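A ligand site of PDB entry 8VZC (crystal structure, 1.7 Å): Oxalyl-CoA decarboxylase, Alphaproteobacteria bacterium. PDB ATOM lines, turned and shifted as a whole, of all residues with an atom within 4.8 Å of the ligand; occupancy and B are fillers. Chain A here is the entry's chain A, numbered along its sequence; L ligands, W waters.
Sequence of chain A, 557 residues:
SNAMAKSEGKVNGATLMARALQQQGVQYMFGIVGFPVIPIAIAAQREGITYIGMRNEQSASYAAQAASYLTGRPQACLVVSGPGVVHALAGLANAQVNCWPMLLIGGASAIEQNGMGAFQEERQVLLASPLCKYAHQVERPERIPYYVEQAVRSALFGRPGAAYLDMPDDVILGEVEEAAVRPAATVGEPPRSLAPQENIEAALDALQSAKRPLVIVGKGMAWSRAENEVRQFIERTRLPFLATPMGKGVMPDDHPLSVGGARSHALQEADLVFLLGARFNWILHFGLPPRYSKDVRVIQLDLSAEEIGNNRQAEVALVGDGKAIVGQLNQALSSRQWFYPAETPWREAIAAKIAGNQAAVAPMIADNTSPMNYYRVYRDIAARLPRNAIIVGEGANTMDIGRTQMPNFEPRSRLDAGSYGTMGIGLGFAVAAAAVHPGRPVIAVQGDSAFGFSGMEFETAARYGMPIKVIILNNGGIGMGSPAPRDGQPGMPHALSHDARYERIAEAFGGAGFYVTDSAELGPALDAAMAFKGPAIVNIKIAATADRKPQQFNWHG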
ATOM      1  N   ASN A  98     -31.893  13.696  -4.313  1.00  0.00           N
ATOM      2  CA  ASN A  98     -32.462  14.993  -3.924  1.00  0.00           C
ATOM      3  C   ASN A  98     -31.525  15.839  -3.063  1.00  0.00           C
ATOM      4  O   ASN A  98     -31.877  16.985  -2.705  1.00  0.00           O
ATOM      5  CB  ASN A  98     -33.782  14.761  -3.161  1.00  0.00           C
ATOM      6  CG  ASN A  98     -34.945  14.381  -4.090  1.00  0.00           C
ATOM      7  OD1 ASN A  98     -35.432  15.206  -4.854  1.00  0.00           O
ATOM      8  ND2 ASN A  98     -35.387  13.125  -4.008  1.00  0.00           N
ATOM      9  N   CYS A  99     -30.353  15.310  -2.689  1.00  0.00           N
ATOM     10  CA  CYS A  99     -29.445  15.999  -1.762  1.00  0.00           C
ATOM     11  C   CYS A  99     -30.130  16.268  -0.432  1.00  0.00           C
ATOM     12  O   CYS A  99     -30.026  17.358   0.139  1.00  0.00           O
ATOM     13  CB  CYS A  99     -28.904  17.308  -2.360  1.00  0.00           C
ATOM     14  SG  CYS A  99     -28.158  17.079  -4.004  1.00  0.00           S
ATOM     15  N   ARG A 159     -22.815  19.037   0.732  1.00  0.00           N
ATOM     16  CA  ARG A 159     -24.005  18.664  -0.004  1.00  0.00           C
ATOM     17  C   ARG A 159     -24.669  17.518   0.756  1.00  0.00           C
ATOM     18  O   ARG A 159     -24.051  16.450   0.904  1.00  0.00           O
ATOM     19  CB  ARG A 159     -23.682  18.228  -1.434  1.00  0.00           C
ATOM     20  CG  ARG A 159     -24.932  17.722  -2.165  1.00  0.00           C
ATOM     21  CD  ARG A 159     -24.602  17.182  -3.556  1.00  0.00           C
ATOM     22  NE  ARG A 159     -24.845  18.195  -4.576  1.00  0.00           N
ATOM     23  CZ  ARG A 159     -24.564  18.038  -5.868  1.00  0.00           C
ATOM     24  NH1 ARG A 159     -23.889  16.987  -6.309  1.00  0.00           N
ATOM     25  NH2 ARG A 159     -24.985  18.956  -6.728  1.00  0.00           N
ATOM     26  N   PRO A 160     -25.907  17.681   1.222  1.00  0.00           N
ATOM     27  CA  PRO A 160     -26.504  16.649   2.087  1.00  0.00           C
ATOM     28  C   PRO A 160     -26.762  15.330   1.351  1.00  0.00           C
ATOM     29  O   PRO A 160     -27.010  15.284   0.141  1.00  0.00           O
ATOM     30  CB  PRO A 160     -27.829  17.284   2.533  1.00  0.00           C
ATOM     31  CG  PRO A 160     -27.542  18.796   2.420  1.00  0.00           C
ATOM     32  CD  PRO A 160     -26.739  18.923   1.193  1.00  0.00           C
ATOM     33  N   GLY A 218     -34.641  27.266  -6.672  1.00  0.00           N
ATOM     34  CA  GLY A 218     -34.695  25.841  -6.482  1.00  0.00           C
ATOM     35  C   GLY A 218     -34.732  25.437  -5.021  1.00  0.00           C
ATOM     36  O   GLY A 218     -34.590  26.249  -4.110  1.00  0.00           O
ATOM     37  N   LYS A 219     -34.940  24.135  -4.817  1.00  0.00           N
ATOM     38  CA  LYS A 219     -35.147  23.632  -3.470  1.00  0.00           C
ATOM     39  C   LYS A 219     -33.880  23.618  -2.622  1.00  0.00           C
ATOM     40  O   LYS A 219     -33.982  23.394  -1.392  1.00  0.00           O
ATOM     41  CB  LYS A 219     -35.800  22.250  -3.489  1.00  0.00           C
ATOM     42  CG  LYS A 219     -34.881  21.083  -3.949  1.00  0.00           C
ATOM     43  CD  LYS A 219     -35.619  19.748  -3.745  1.00  0.00           C
ATOM     44  CE  LYS A 219     -34.753  18.465  -4.125  1.00  0.00           C
ATOM     45  NZ  LYS A 219     -34.793  18.200  -5.586  1.00  0.00           N
ATOM     46  N   GLY A 220     -32.701  23.869  -3.209  1.00  0.00           N
ATOM     47  CA  GLY A 220     -31.516  24.102  -2.419  1.00  0.00           C
ATOM     48  C   GLY A 220     -31.636  25.378  -1.600  1.00  0.00           C
ATOM     49  O   GLY A 220     -31.066  25.480  -0.502  1.00  0.00           O
ATOM     50  N   TRP A 223     -33.752  24.198   1.361  1.00  0.00           N
ATOM     51  CA  TRP A 223     -32.877  23.505   2.307  1.00  0.00           C
ATOM     52  C   TRP A 223     -32.011  24.500   3.099  1.00  0.00           C
ATOM     53  O   TRP A 223     -31.872  24.381   4.326  1.00  0.00           O
ATOM     54  CB  TRP A 223     -31.997  22.472   1.582  1.00  0.00           C
ATOM     55  CG  TRP A 223     -30.935  21.973   2.523  1.00  0.00           C
ATOM     56  CD1 TRP A 223     -29.620  22.315   2.532  1.00  0.00           C
ATOM     57  CD2 TRP A 223     -31.138  21.131   3.663  1.00  0.00           C
ATOM     58  NE1 TRP A 223     -28.974  21.725   3.605  1.00  0.00           N
ATOM     59  CE2 TRP A 223     -29.886  21.004   4.313  1.00  0.00           C
ATOM     60  CE3 TRP A 223     -32.259  20.487   4.199  1.00  0.00           C
ATOM     61  CZ2 TRP A 223     -29.730  20.247   5.466  1.00  0.00           C
ATOM     62  CZ3 TRP A 223     -32.098  19.722   5.349  1.00  0.00           C
ATOM     63  CH2 TRP A 223     -30.843  19.606   5.970  1.00  0.00           C
ATOM     64  N   SER A 224     -31.436  25.493   2.428  1.00  0.00           N
ATOM     65  CA  SER A 224     -30.557  26.467   3.047  1.00  0.00           C
ATOM     66  C   SER A 224     -31.289  27.432   3.990  1.00  0.00           C
ATOM     67  O   SER A 224     -30.604  28.177   4.711  1.00  0.00           O
ATOM     68  CB  SER A 224     -29.847  27.268   1.947  1.00  0.00           C
ATOM     69  OG  SER A 224     -28.873  28.154   2.487  1.00  0.00           O
ATOM     70  N   THR A 244     -38.931  26.141  -9.013  1.00  0.00           N
ATOM     71  CA  THR A 244     -38.879  24.719  -9.351  1.00  0.00           C
ATOM     72  C   THR A 244     -39.983  24.016  -8.561  1.00  0.00           C
ATOM     73  O   THR A 244     -40.615  24.633  -7.699  1.00  0.00           O
ATOM     74  CB  THR A 244     -37.508  24.148  -9.013  1.00  0.00           C
ATOM     75  OG1 THR A 244     -37.326  24.171  -7.588  1.00  0.00           O
ATOM     76  CG2 THR A 244     -36.386  24.908  -9.722  1.00  0.00           C
ATOM     77  N   GLY A 247     -38.995  24.071  -5.017  1.00  0.00           N
ATOM     78  CA  GLY A 247     -38.658  25.445  -4.721  1.00  0.00           C
ATOM     79  C   GLY A 247     -39.863  26.358  -4.551  1.00  0.00           C
ATOM     80  O   GLY A 247     -39.688  27.479  -4.059  1.00  0.00           O
ATOM     81  N   GLY A 277     -29.598  27.498  -6.251  1.00  0.00           N
ATOM     82  CA  GLY A 277     -29.761  26.205  -5.617  1.00  0.00           C
ATOM     83  C   GLY A 277     -30.687  25.292  -6.401  1.00  0.00           C
ATOM     84  O   GLY A 277     -31.601  24.675  -5.837  1.00  0.00           O
ATOM     85  N   ALA A 278     -30.474  25.245  -7.709  1.00  0.00           N
ATOM     86  CA  ALA A 278     -31.234  24.410  -8.622  1.00  0.00           C
ATOM     87  C   ALA A 278     -30.283  23.903  -9.698  1.00  0.00           C
ATOM     88  O   ALA A 278     -29.391  24.646 -10.138  1.00  0.00           O
ATOM     89  CB  ALA A 278     -32.367  25.212  -9.289  1.00  0.00           C
ATOM     90  N   ARG A 279     -30.481  22.670 -10.146  1.00  0.00           N
ATOM     91  CA  ARG A 279     -29.541  22.094 -11.100  1.00  0.00           C
ATOM     92  C   ARG A 279     -30.111  22.095 -12.519  1.00  0.00           C
ATOM     93  O   ARG A 279     -31.318  21.962 -12.723  1.00  0.00           O
ATOM     94  CB  ARG A 279     -29.165  20.656 -10.723  1.00  0.00           C
ATOM     95  CG  ARG A 279     -28.361  20.525  -9.449  1.00  0.00           C
ATOM     96  CD  ARG A 279     -28.115  19.029  -9.091  1.00  0.00           C
ATOM     97  NE  ARG A 279     -29.353  18.482  -8.544  1.00  0.00           N
ATOM     98  CZ  ARG A 279     -29.477  17.320  -7.911  1.00  0.00           C
ATOM     99  NH1 ARG A 279     -28.455  16.468  -7.816  1.00  0.00           N
ATOM    100  NH2 ARG A 279     -30.651  17.020  -7.346  1.00  0.00           N
ATOM    101  N   ASN A 281     -30.425  19.759 -14.381  1.00  0.00           N
ATOM    102  CA  ASN A 281     -30.739  18.365 -14.686  1.00  0.00           C
ATOM    103  C   ASN A 281     -32.033  18.330 -15.507  1.00  0.00           C
ATOM    104  O   ASN A 281     -32.435  19.362 -16.088  1.00  0.00           O
ATOM    105  CB  ASN A 281     -30.786  17.552 -13.392  1.00  0.00           C
ATOM    106  CG  ASN A 281     -32.002  17.897 -12.517  1.00  0.00           C
ATOM    107  OD1 ASN A 281     -32.714  18.856 -12.795  1.00  0.00           O
ATOM    108  ND2 ASN A 281     -32.239  17.102 -11.475  1.00  0.00           N
ATOM    109  N   ILE A 283     -35.171  18.331 -14.651  1.00  0.00           N
ATOM    110  CA  ILE A 283     -36.277  19.205 -14.217  1.00  0.00           C
ATOM    111  C   ILE A 283     -36.188  20.579 -14.862  1.00  0.00           C
ATOM    112  O   ILE A 283     -37.220  21.237 -15.121  1.00  0.00           O
ATOM    113  CB  ILE A 283     -36.325  19.273 -12.677  1.00  0.00           C
ATOM    114  CG1 ILE A 283     -37.146  18.093 -12.134  1.00  0.00           C
ATOM    115  CG2 ILE A 283     -36.885  20.665 -12.155  1.00  0.00           C
ATOM    116  CD1 ILE A 283     -37.002  17.857 -10.641  1.00  0.00           C
ATOM    117  N   LEU A 284     -34.972  21.056 -15.118  1.00  0.00           N
ATOM    118  CA  LEU A 284     -34.760  22.319 -15.829  1.00  0.00           C
ATOM    119  C   LEU A 284     -34.274  22.097 -17.256  1.00  0.00           C
ATOM    120  O   LEU A 284     -33.679  23.006 -17.854  1.00  0.00           O
ATOM    121  CB  LEU A 284     -33.793  23.200 -15.060  1.00  0.00           C
ATOM    122  CG  LEU A 284     -34.402  23.822 -13.796  1.00  0.00           C
ATOM    123  CD1 LEU A 284     -33.366  24.686 -13.033  1.00  0.00           C
ATOM    124  CD2 LEU A 284     -35.651  24.653 -14.164  1.00  0.00           C
ATOM    125  N   LEU A 301     -25.534  29.603  -8.442  1.00  0.00           N
ATOM    126  CA  LEU A 301     -25.276  29.538  -7.019  1.00  0.00           C
ATOM    127  C   LEU A 301     -25.558  28.114  -6.567  1.00  0.00           C
ATOM    128  O   LEU A 301     -26.714  27.690  -6.519  1.00  0.00           O
ATOM    129  CB  LEU A 301     -26.163  30.546  -6.266  1.00  0.00           C
ATOM    130  CG  LEU A 301     -25.819  30.869  -4.809  1.00  0.00           C
ATOM    131  CD1 LEU A 301     -26.766  31.996  -4.238  1.00  0.00           C
ATOM    132  CD2 LEU A 301     -25.821  29.652  -3.858  1.00  0.00           C
ATOM    133  N   ASP A 302     -24.493  27.373  -6.217  1.00  0.00           N
ATOM    134  CA  ASP A 302     -24.639  26.044  -5.667  1.00  0.00           C
ATOM    135  C   ASP A 302     -23.598  25.827  -4.590  1.00  0.00           C
ATOM    136  O   ASP A 302     -22.480  26.328  -4.687  1.00  0.00           O
ATOM    137  CB  ASP A 302     -24.471  24.969  -6.765  1.00  0.00           C
ATOM    138  CG  ASP A 302     -25.131  23.659  -6.384  1.00  0.00           C
ATOM    139  OD1 ASP A 302     -24.641  23.025  -5.424  1.00  0.00           O
ATOM    140  OD2 ASP A 302     -26.130  23.287  -7.041  1.00  0.00           O
ATOM    141  N   LEU A 303     -23.958  25.079  -3.546  1.00  0.00           N
ATOM    142  CA  LEU A 303     -22.968  24.688  -2.547  1.00  0.00           C
ATOM    143  C   LEU A 303     -21.888  23.781  -3.150  1.00  0.00           C
ATOM    144  O   LEU A 303     -20.755  23.757  -2.663  1.00  0.00           O
ATOM    145  CB  LEU A 303     -23.683  24.001  -1.360  1.00  0.00           C
ATOM    146  CG  LEU A 303     -22.949  23.417  -0.146  1.00  0.00           C
ATOM    147  CD1 LEU A 303     -23.871  23.230   1.050  1.00  0.00           C
ATOM    148  CD2 LEU A 303     -22.412  22.021  -0.509  1.00  0.00           C
ATOM    149  N   SER A 304     -22.220  23.037  -4.208  1.00  0.00           N
ATOM    150  CA  SER A 304     -21.350  22.015  -4.795  1.00  0.00           C
ATOM    151  C   SER A 304     -20.507  22.613  -5.921  1.00  0.00           C
ATOM    152  O   SER A 304     -21.043  22.922  -7.002  1.00  0.00           O
ATOM    153  CB  SER A 304     -22.188  20.867  -5.322  1.00  0.00           C
ATOM    154  OG  SER A 304     -21.338  19.876  -5.930  1.00  0.00           O
ATOM    155  N   GLU A 307     -20.783  20.847  -9.313  1.00  0.00           N
ATOM    156  CA  GLU A 307     -22.004  21.045 -10.090  1.00  0.00           C
ATOM    157  C   GLU A 307     -21.910  22.243 -11.042  1.00  0.00           C
ATOM    158  O   GLU A 307     -22.679  22.310 -12.014  1.00  0.00           O
ATOM    159  CB  GLU A 307     -23.177  21.252  -9.117  1.00  0.00           C
ATOM    160  CG  GLU A 307     -24.571  21.210  -9.724  1.00  0.00           C
ATOM    161  CD  GLU A 307     -24.881  19.838 -10.315  1.00  0.00           C
ATOM    162  OE1 GLU A 307     -24.438  18.836  -9.715  1.00  0.00           O
ATOM    163  OE2 GLU A 307     -25.564  19.792 -11.379  1.00  0.00           O
ATOM    164  N   GLY A 320     -21.045  28.216  -2.685  1.00  0.00           N
ATOM    165  CA  GLY A 320     -21.211  28.409  -1.262  1.00  0.00           C
ATOM    166  C   GLY A 320     -22.684  28.312  -0.899  1.00  0.00           C
ATOM    167  O   GLY A 320     -23.494  27.826  -1.678  1.00  0.00           O
ATOM    168  N   ASP A 321     -22.997  28.803   0.302  1.00  0.00           N
ATOM    169  CA  ASP A 321     -24.313  28.626   0.899  1.00  0.00           C
ATOM    170  C   ASP A 321     -25.318  29.610   0.309  1.00  0.00           C
ATOM    171  O   ASP A 321     -25.028  30.798   0.127  1.00  0.00           O
ATOM    172  CB  ASP A 321     -24.232  28.827   2.412  1.00  0.00           C
ATOM    173  CG  ASP A 321     -25.579  28.706   3.079  1.00  0.00           C
ATOM    174  OD1 ASP A 321     -26.134  27.611   3.090  1.00  0.00           O
ATOM    175  OD2 ASP A 321     -26.099  29.723   3.608  1.00  0.00           O
ATOM    176  N   GLY A 322     -26.527  29.107   0.059  1.00  0.00           N
ATOM    177  CA  GLY A 322     -27.548  29.938  -0.571  1.00  0.00           C
ATOM    178  C   GLY A 322     -27.918  31.146   0.271  1.00  0.00           C
ATOM    179  O   GLY A 322     -27.963  32.254  -0.237  1.00  0.00           O
ATOM    180  N   SER A 419     -36.499  14.733  -7.535  1.00  0.00           N
ATOM    181  CA  SER A 419     -35.499  14.668  -8.590  1.00  0.00           C
ATOM    182  C   SER A 419     -35.336  13.251  -9.156  1.00  0.00           C
ATOM    183  O   SER A 419     -34.757  13.089 -10.224  1.00  0.00           O
ATOM    184  CB  SER A 419     -34.141  15.185  -8.075  1.00  0.00           C
ATOM    185  OG  SER A 419     -34.223  16.568  -7.666  1.00  0.00           O
HETATM  186  P1  LIG L   1     -34.600  21.606  -7.966  1.00  0.00           P
HETATM  187  O1  LIG L   1     -35.215  20.242  -8.124  1.00  0.00           O
HETATM  188  O2  LIG L   1     -34.230  22.230  -9.288  1.00  0.00           O
HETATM  189  O3  LIG L   1     -35.352  22.558  -7.095  1.00  0.00           O
HETATM  190  P2  LIG L   1     -32.046  20.380  -7.367  1.00  0.00           P
HETATM  191  O4  LIG L   1     -32.346  19.252  -6.412  1.00  0.00           O
HETATM  192  O5  LIG L   1     -31.836  20.147  -8.847  1.00  0.00           O
HETATM  193  O6  LIG L   1     -33.214  21.489  -7.142  1.00  0.00           O
HETATM  194  O7  LIG L   1     -30.774  21.214  -6.872  1.00  0.00           O
HETATM  195  C1  LIG L   1     -30.567  21.502  -5.480  1.00  0.00           C
HETATM  196  C2  LIG L   1     -29.125  21.955  -5.358  1.00  0.00           C
HETATM  197  O8  LIG L   1     -29.008  22.649  -4.123  1.00  0.00           O
HETATM  198  C3  LIG L   1     -28.090  20.819  -5.366  1.00  0.00           C
HETATM  199  O9  LIG L   1     -27.236  20.991  -6.489  1.00  0.00           O
HETATM  200  C4  LIG L   1     -27.338  21.029  -4.051  1.00  0.00           C
HETATM  201  O10 LIG L   1     -25.916  20.870  -4.157  1.00  0.00           O
HETATM  202  C5  LIG L   1     -27.666  22.484  -3.716  1.00  0.00           C
HETATM  203  N1  LIG L   1     -27.545  22.821  -2.297  1.00  0.00           N
HETATM  204  C6  LIG L   1     -27.686  22.004  -1.236  1.00  0.00           C
HETATM  205  N2  LIG L   1     -27.533  22.708  -0.079  1.00  0.00           N
HETATM  206  C7  LIG L   1     -27.254  23.974  -0.418  1.00  0.00           C
HETATM  207  C8  LIG L   1     -26.976  25.239   0.302  1.00  0.00           C
HETATM  208  N3  LIG L   1     -26.921  25.309   1.647  1.00  0.00           N
HETATM  209  N4  LIG L   1     -26.778  26.325  -0.444  1.00  0.00           N
HETATM  210  C9  LIG L   1     -26.822  26.312  -1.799  1.00  0.00           C
HETATM  211  N5  LIG L   1     -27.071  25.212  -2.532  1.00  0.00           N
HETATM  212  C10 LIG L   1     -27.297  24.045  -1.881  1.00  0.00           C
HETATM  213  O   HOH W   1     -36.976  18.533  -7.149  1.00  0.00           O
HETATM  214  O   HOH W   2     -29.892  20.045  -0.250  1.00  0.00           O
HETATM  215  O   HOH W   3     -33.487  21.176 -11.436  1.00  0.00           O
HETATM  216  O   HOH W   4     -33.750  18.455  -9.367  1.00  0.00           O
HETATM  217  O   HOH W   5     -26.427  23.495   3.793  1.00  0.00           O
HETATM  218  O   HOH W   6     -37.715  20.864  -6.626  1.00  0.00           O
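Residues that only touch the ligand: Gly 277 (3.4 Å), Gly 220 (3.4 Å), Trp 223 (3.4 Å), Gly 218 (3.4 Å), Ser 419 (3.5 Å), Ala 278 (3.5 Å), Ser 224 (3.5 Å), Gly 320 (3.7 Å), Ile 283 (3.9 Å), Ser 304 (3.9 Å) and Cys 99 (3.98 Å).
Hydrophobic or aromatic side chains that line the ligand: Trp 223, Ala 278, Ile 283 and Leu 303.
Within 4 Å of the ligand: Cys 99, Arg 159, Gly 218, Lys 219, Gly 220, Trp 223, Ser 224, Thr 244, Gly 277, Ala 278, Arg 279, Ile 283, Asp 302, Leu 303, Ser 304, Gly 320, Asp 321, Gly 322 and Ser 419.
The nearest printed residue that does not touch the ligand is Pro 160 (4.04 Å).
OD2 of Asp 302 is in hydrogen-bond range of O9 of the ligand (2.6 Å).
An oxygen (O3) of the ligand is in hydrogen-bond range of the side-chain hydroxyl of Thr 244 (2.6 Å).
O3 of the ligand lies within hydrogen-bond range of N of Lys 219.
The side-chain amino group (NZ) of Lys 219 lies within salt-bridge range of an oxygen (O4) of the ligand, at 2.8 Å.
The guanidinium group (NH2) of Arg 279 lies within salt-bridge range of an oxygen (O4) of the ligand.
N of Leu 303 is in hydrogen-bond range of N5 of the ligand (3.3 Å).
A nitrogen (N3) of the ligand lies within hydrogen-bond range of the side-chain carboxylate of Asp 321, 2.8 Å away.
N of Arg 279 lies within hydrogen-bond range of O5 of the ligand (3.1 Å).
NE of Arg 159 sits at hydrogen-bond distance from O10 of the ligand, 2.9 Å away.
N of Gly 322 lies within hydrogen-bond range of N4 of the ligand, 2.8 Å away.
The guanidinium group (NH2) of Arg 159 lies within salt-bridge range of the side-chain carboxylate (OE1) of Glu 307.
O of Arg 279 lies close to OD1 of Asn 281 (3.4 Å).
OD1 of Asp 302 sits at hydrogen-bond distance from N of Ser 304 (2.7 Å).
The backbone carbonyl oxygen of Gly 320 sits close to the backbone NH of Leu 303 (3.4 Å).
NE of Arg 159 is in hydrogen-bond range of SG of Cys 99.
The backbone carbonyl oxygen (O) of Asp 302 lies within hydrogen-bond range of the backbone NH (N) of Gly 320.
The side-chain hydroxyl (OG) of Ser 224 lies within hydrogen-bond range of the side-chain carboxylate (OD1) of Asp 321.
N of Gly 277 is in hydrogen-bond range of O of Leu 301 (2.9 Å).
Water W3 lies within hydrogen-bond range of an oxygen (O2) of the ligand (2.5 Å), the backbone carbonyl oxygen of Arg 279 (2.6 Å) and the side-chain amide oxygen of Asn 281 (2.8 Å).
Water W4 lies within hydrogen-bond range of the side-chain hydroxyl (OG) of Ser 419, an oxygen (O5) of the ligand and the side-chain amide nitrogen (ND2) of Asn 281.
Water W1 lies within hydrogen-bond range of O1 of the ligand (2.6 Å), NZ of Lys 219 (2.7 Å) and OG of Ser 419 (3.4 Å).
Water W5 bridges N3 of the ligand (2.9 Å) and NE1 of Trp 223 (3.1 Å).
Water W6 lies within hydrogen-bond range of O3 of the ligand and OG1 of Thr 244.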
